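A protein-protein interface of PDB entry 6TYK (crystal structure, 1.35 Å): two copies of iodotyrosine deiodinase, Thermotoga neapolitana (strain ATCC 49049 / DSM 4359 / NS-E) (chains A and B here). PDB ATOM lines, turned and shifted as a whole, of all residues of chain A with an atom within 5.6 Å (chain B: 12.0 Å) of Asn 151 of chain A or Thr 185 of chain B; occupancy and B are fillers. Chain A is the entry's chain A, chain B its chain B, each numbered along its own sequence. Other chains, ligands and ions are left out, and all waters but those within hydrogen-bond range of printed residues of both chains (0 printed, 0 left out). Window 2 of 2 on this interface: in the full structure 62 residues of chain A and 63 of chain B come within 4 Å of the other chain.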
ATOM      1  N   LEU A  49       4.702  -3.594   6.159  1.00  0.00           N
ATOM      2  CA  LEU A  49       5.763  -4.462   6.639  1.00  0.00           C
ATOM      3  C   LEU A  49       7.058  -3.956   6.029  1.00  0.00           C
ATOM      4  O   LEU A  49       7.201  -3.915   4.808  1.00  0.00           O
ATOM      5  CB  LEU A  49       5.513  -5.908   6.213  1.00  0.00           C
ATOM      6  CG  LEU A  49       6.545  -6.937   6.665  1.00  0.00           C
ATOM      7  CD1 LEU A  49       6.561  -7.075   8.182  1.00  0.00           C
ATOM      8  CD2 LEU A  49       6.281  -8.284   6.012  1.00  0.00           C
ATOM      9  N   LEU A  56      16.443 -12.158   4.413  1.00  0.00           N
ATOM     10  CA  LEU A  56      15.047 -12.151   3.997  1.00  0.00           C
ATOM     11  C   LEU A  56      14.867 -11.450   2.650  1.00  0.00           C
ATOM     12  O   LEU A  56      14.113 -11.924   1.804  1.00  0.00           O
ATOM     13  CB  LEU A  56      14.172 -11.509   5.069  1.00  0.00           C
ATOM     14  CG  LEU A  56      12.688 -11.417   4.753  1.00  0.00           C
ATOM     15  CD1 LEU A  56      12.119 -12.790   4.457  1.00  0.00           C
ATOM     16  CD2 LEU A  56      11.990 -10.792   5.955  1.00  0.00           C
ATOM     17  N   VAL A 146       5.724 -14.943  -1.702  1.00  0.00           N
ATOM     18  CA  VAL A 146       6.307 -13.875  -0.906  1.00  0.00           C
ATOM     19  C   VAL A 146       5.526 -13.728   0.394  1.00  0.00           C
ATOM     20  O   VAL A 146       6.112 -13.555   1.462  1.00  0.00           O
ATOM     21  CB  VAL A 146       6.353 -12.545  -1.684  1.00  0.00           C
ATOM     22  CG1 VAL A 146       6.865 -11.432  -0.790  1.00  0.00           C
ATOM     23  CG2 VAL A 146       7.234 -12.696  -2.922  1.00  0.00           C
ATOM     24  N   GLU A 147       4.203 -13.827   0.306  1.00  0.00           N
ATOM     25  CA  GLU A 147       3.361 -13.762   1.497  1.00  0.00           C
ATOM     26  C   GLU A 147       3.774 -14.800   2.528  1.00  0.00           C
ATOM     27  O   GLU A 147       3.823 -14.510   3.721  1.00  0.00           O
ATOM     28  CB  GLU A 147       1.892 -13.965   1.136  1.00  0.00           C
ATOM     29  CG  GLU A 147       1.230 -12.746   0.520  1.00  0.00           C
ATOM     30  CD  GLU A 147      -0.243 -12.975   0.263  1.00  0.00           C
ATOM     31  OE1 GLU A 147      -0.703 -14.121   0.408  1.00  0.00           O
ATOM     32  OE2 GLU A 147      -0.950 -12.020  -0.084  1.00  0.00           O
ATOM     33  N   LYS A 148       4.072 -16.008   2.061  1.00  0.00           N
ATOM     34  CA  LYS A 148       4.431 -17.089   2.968  1.00  0.00           C
ATOM     35  C   LYS A 148       5.780 -16.815   3.625  1.00  0.00           C
ATOM     36  O   LYS A 148       5.979 -17.125   4.802  1.00  0.00           O
ATOM     37  CB  LYS A 148       4.450 -18.435   2.233  1.00  0.00           C
ATOM     38  CG  LYS A 148       4.789 -19.629   3.115  1.00  0.00           C
ATOM     39  CD  LYS A 148       4.931 -20.888   2.283  1.00  0.00           C
ATOM     40  CE  LYS A 148       5.427 -22.056   3.120  1.00  0.00           C
ATOM     41  NZ  LYS A 148       5.836 -23.201   2.266  1.00  0.00           N
ATOM     42  N   LEU A 149       6.700 -16.229   2.862  1.00  0.00           N
ATOM     43  CA  LEU A 149       8.031 -15.919   3.376  1.00  0.00           C
ATOM     44  C   LEU A 149       7.978 -15.017   4.594  1.00  0.00           C
ATOM     45  O   LEU A 149       8.824 -15.110   5.479  1.00  0.00           O
ATOM     46  CB  LEU A 149       8.897 -15.254   2.305  1.00  0.00           C
ATOM     47  CG  LEU A 149       9.499 -16.146   1.234  1.00  0.00           C
ATOM     48  CD1 LEU A 149      10.295 -15.280   0.269  1.00  0.00           C
ATOM     49  CD2 LEU A 149      10.386 -17.191   1.883  1.00  0.00           C
ATOM     50  N   VAL A 150       6.989 -14.132   4.632  1.00  0.00           N
ATOM     51  CA  VAL A 150       6.902 -13.162   5.720  1.00  0.00           C
ATOM     52  C   VAL A 150       5.783 -13.500   6.710  1.00  0.00           C
ATOM     53  O   VAL A 150       5.409 -12.679   7.546  1.00  0.00           O
ATOM     54  CB  VAL A 150       6.796 -11.698   5.205  1.00  0.00           C
ATOM     55  CG1 VAL A 150       8.024 -11.335   4.367  1.00  0.00           C
ATOM     56  CG2 VAL A 150       5.519 -11.490   4.406  1.00  0.00           C
ATOM     57  N   ASN A 151       5.261 -14.719   6.610  1.00  0.00           N
ATOM     58  CA  ASN A 151       4.237 -15.199   7.535  1.00  0.00           C
ATOM     59  C   ASN A 151       2.985 -14.328   7.528  1.00  0.00           C
ATOM     60  O   ASN A 151       2.433 -13.996   8.579  1.00  0.00           O
ATOM     61  CB  ASN A 151       4.800 -15.288   8.952  1.00  0.00           C
ATOM     62  CG  ASN A 151       6.078 -16.095   9.020  1.00  0.00           C
ATOM     63  OD1 ASN A 151       6.232 -17.098   8.327  1.00  0.00           O
ATOM     64  ND2 ASN A 151       7.007 -15.657   9.859  1.00  0.00           N
ATOM     65  N   THR A 152       2.538 -13.958   6.335  1.00  0.00           N
ATOM     66  CA  THR A 152       1.364 -13.113   6.185  1.00  0.00           C
ATOM     67  C   THR A 152       0.140 -13.803   6.768  1.00  0.00           C
ATOM     68  O   THR A 152      -0.141 -14.957   6.438  1.00  0.00           O
ATOM     69  CB  THR A 152       1.106 -12.818   4.704  1.00  0.00           C
ATOM     70  OG1 THR A 152       2.281 -12.241   4.129  1.00  0.00           O
ATOM     71  CG2 THR A 152      -0.055 -11.857   4.538  1.00  0.00           C
ATOM     72  N   PRO A 153      -0.592 -13.103   7.647  1.00  0.00           N
ATOM     73  CA  PRO A 153      -1.837 -13.676   8.168  1.00  0.00           C
ATOM     74  C   PRO A 153      -2.882 -13.764   7.063  1.00  0.00           C
ATOM     75  O   PRO A 153      -2.838 -12.988   6.114  1.00  0.00           O
ATOM     76  CB  PRO A 153      -2.270 -12.683   9.251  1.00  0.00           C
ATOM     77  CG  PRO A 153      -1.560 -11.434   8.961  1.00  0.00           C
ATOM     78  CD  PRO A 153      -0.309 -11.767   8.198  1.00  0.00           C
ATOM     79  N   ILE B 180       0.907   1.665  12.600  1.00  0.00           N
ATOM     80  CA  ILE B 180       1.682   0.701  13.364  1.00  0.00           C
ATOM     81  C   ILE B 180       2.385  -0.237  12.397  1.00  0.00           C
ATOM     82  O   ILE B 180       1.771  -1.098  11.767  1.00  0.00           O
ATOM     83  CB  ILE B 180       0.808  -0.099  14.343  1.00  0.00           C
ATOM     84  CG1 ILE B 180       0.155   0.845  15.355  1.00  0.00           C
ATOM     85  CG2 ILE B 180       1.644  -1.152  15.057  1.00  0.00           C
ATOM     86  CD1 ILE B 180      -0.800   0.156  16.311  1.00  0.00           C
ATOM     87  N   VAL B 181       3.687  -0.058  12.276  1.00  0.00           N
ATOM     88  CA  VAL B 181       4.447  -0.816  11.300  1.00  0.00           C
ATOM     89  C   VAL B 181       4.901  -2.143  11.886  1.00  0.00           C
ATOM     90  O   VAL B 181       4.954  -2.315  13.102  1.00  0.00           O
ATOM     91  CB  VAL B 181       5.665  -0.021  10.807  1.00  0.00           C
ATOM     92  CG1 VAL B 181       6.439  -0.826   9.788  1.00  0.00           C
ATOM     93  CG2 VAL B 181       5.215   1.292  10.201  1.00  0.00           C
ATOM     94  N   ARG B 182       5.199  -3.085  11.002  1.00  0.00           N
ATOM     95  CA  ARG B 182       5.854  -4.318  11.391  1.00  0.00           C
ATOM     96  C   ARG B 182       7.175  -4.389  10.653  1.00  0.00           C
ATOM     97  O   ARG B 182       7.351  -3.724   9.633  1.00  0.00           O
ATOM     98  CB  ARG B 182       4.972  -5.521  11.059  1.00  0.00           C
ATOM     99  CG  ARG B 182       3.764  -5.658  11.973  1.00  0.00           C
ATOM    100  CD  ARG B 182       2.873  -6.797  11.509  1.00  0.00           C
ATOM    101  NE  ARG B 182       1.829  -7.125  12.472  1.00  0.00           N
ATOM    102  CZ  ARG B 182       0.593  -6.638  12.427  1.00  0.00           C
ATOM    103  NH1 ARG B 182       0.242  -5.785  11.470  1.00  0.00           N
ATOM    104  NH2 ARG B 182      -0.294  -7.001  13.341  1.00  0.00           N
ATOM    105  N   TYR B 183       8.105  -5.187  11.166  1.00  0.00           N
ATOM    106  CA  TYR B 183       9.411  -5.341  10.536  1.00  0.00           C
ATOM    107  C   TYR B 183       9.690  -6.774  10.158  1.00  0.00           C
ATOM    108  O   TYR B 183       9.494  -7.696  10.954  1.00  0.00           O
ATOM    109  CB  TYR B 183      10.518  -4.869  11.473  1.00  0.00           C
ATOM    110  CG  TYR B 183      10.439  -3.403  11.770  1.00  0.00           C
ATOM    111  CD1 TYR B 183       9.646  -2.928  12.814  1.00  0.00           C
ATOM    112  CD2 TYR B 183      11.135  -2.484  10.999  1.00  0.00           C
ATOM    113  CE1 TYR B 183       9.560  -1.581  13.080  1.00  0.00           C
ATOM    114  CE2 TYR B 183      11.054  -1.136  11.259  1.00  0.00           C
ATOM    115  CZ  TYR B 183      10.264  -0.689  12.300  1.00  0.00           C
ATOM    116  OH  TYR B 183      10.171   0.656  12.563  1.00  0.00           O
ATOM    117  N   ASN B 184      10.177  -6.925   8.937  1.00  0.00           N
ATOM    118  CA  ASN B 184      10.644  -8.188   8.383  1.00  0.00           C
ATOM    119  C   ASN B 184       9.576  -9.255   8.184  1.00  0.00           C
ATOM    120  O   ASN B 184       9.263  -9.603   7.043  1.00  0.00           O
ATOM    121  CB  ASN B 184      11.860  -8.700   9.151  1.00  0.00           C
ATOM    122  CG  ASN B 184      13.064  -7.823   8.932  1.00  0.00           C
ATOM    123  OD1 ASN B 184      13.377  -7.476   7.796  1.00  0.00           O
ATOM    124  ND2 ASN B 184      13.718  -7.416  10.009  1.00  0.00           N
ATOM    125  N   THR B 185       9.004  -9.757   9.274  1.00  0.00           N
ATOM    126  CA  THR B 185       7.954 -10.757   9.162  1.00  0.00           C
ATOM    127  C   THR B 185       6.859 -10.476  10.182  1.00  0.00           C
ATOM    128  O   THR B 185       7.076  -9.755  11.156  1.00  0.00           O
ATOM    129  CB  THR B 185       8.489 -12.196   9.377  1.00  0.00           C
ATOM    130  OG1 THR B 185       8.815 -12.381  10.761  1.00  0.00           O
ATOM    131  CG2 THR B 185       9.724 -12.460   8.511  1.00  0.00           C
ATOM    132  N   PHE B 186       5.680 -11.036   9.945  1.00  0.00           N
ATOM    133  CA  PHE B 186       4.640 -11.064  10.961  1.00  0.00           C
ATOM    134  C   PHE B 186       5.010 -12.078  12.043  1.00  0.00           C
ATOM    135  O   PHE B 186       4.968 -11.757  13.229  1.00  0.00           O
ATOM    136  CB  PHE B 186       3.287 -11.409  10.338  1.00  0.00           C
ATOM    137  CG  PHE B 186       2.786 -10.381   9.355  1.00  0.00           C
ATOM    138  CD1 PHE B 186       3.179 -10.422   8.025  1.00  0.00           C
ATOM    139  CD2 PHE B 186       1.921  -9.376   9.759  1.00  0.00           C
ATOM    140  CE1 PHE B 186       2.716  -9.480   7.118  1.00  0.00           C
ATOM    141  CE2 PHE B 186       1.458  -8.436   8.859  1.00  0.00           C
ATOM    142  CZ  PHE B 186       1.852  -8.490   7.537  1.00  0.00           C
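No position is printed for both chains.
CA of Leu 49 of chain A touches O of Arg 182 of chain B (3.5 Å).
CD2 of Leu 49 of chain A touches O of Asn 184 of chain B (3.4 Å).
CD1 of Leu 49 of chain A touches N of Thr 185 of chain B, at 3.8 Å.
Phe 186 of chain B touches Leu 49 of chain A (CE1 to CD2, 3.9 Å).
Leu 56 of chain A touches Thr 185 of chain B.
Val 150 of chain A touches Asn 184 of chain B.
O of Val 150 of chain A touches CA of Thr 185 of chain B, at 3.6 Å.
Phe 186 of chain B touches Asn 151 of chain A (CB to O, 3.2 Å).
Thr 152 of chain A touches Phe 186 of chain B.
Pro 153 of chain A touches Phe 186 of chain B.
Printed residues of chain B that touch a printed residue of chain A: Arg 182, Tyr 183, Asn 184, Thr 185 and Phe 186.
Hydrophobic or aromatic side chains of chain B that line the printed part of chain A: Phe 186.
Printed residues of chain A that touch a printed residue of chain B: Leu 49, Leu 56, Val 150, Asn 151, Thr 152 and Pro 153.
Hydrophobic or aromatic side chains of chain A within 4 Å of the printed part of chain B: Leu 49, Leu 56, Val 150 and Pro 153.
Along chain A the printed residues that touch a printed residue of chain B span positions 49 to 153.
Among the printed residues, no Asp or Glu carboxylate lies within 4 Å of a Lys or Arg side-chain nitrogen of the other chain.
O of Val 150 of chain A is in hydrogen-bond range of N of Phe 186 of chain B, at 2.9 Å.
Printed residues of chain A within 4 Å of Thr 185 of chain B: Leu 49 (3.8 Å), Leu 56 (3.8 Å), Val 150 (3.6 Å) and Asn 151 (3.8 Å).
Val 150 of chain A touches just these residues of chain B: Asn 184, Thr 185 and Phe 186.
Of chain B, only Phe 186 (3.6 Å) comes within 4 Å of Pro 153 of chain A.
Printed residues of chain A within 4 Å of Arg 182 of chain B: Leu 49.
Of the printed residues of chain A, Tyr 183 of chain B touches Leu 49.
Of the printed residues of chain B, Leu 56 of chain A touches Asn 184 and Thr 185.
Of the printed residues of chain A, Asn 184 of chain B touches Leu 49 (3.4 Å), Leu 56 (3.2 Å) and Val 150 (3.4 Å).
Of the printed residues of chain A, Phe 186 of chain B touches Leu 49, Val 150, Asn 151, Thr 152 and Pro 153.
Leu 149 of chain A touches none of the printed residues of chain B.
Val 181 of chain B touches none of the printed residues of chain A.
The nearest printed residue of chain B that does not touch Asn 151 of chain A is Asn 184 of chain B (6.5 Å).
The nearest printed residue of chain A that does not touch Thr 185 of chain B is Leu 149 of chain A (4.1 Å).
The nearest printed residue of chain A that does not touch Asn 184 of chain B is Leu 149 of chain A (5.7 Å).
The backbone carbonyl oxygen of Glu 147 of chain A is in hydrogen-bond range of the side-chain hydroxyl of Thr 152 of chain A.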
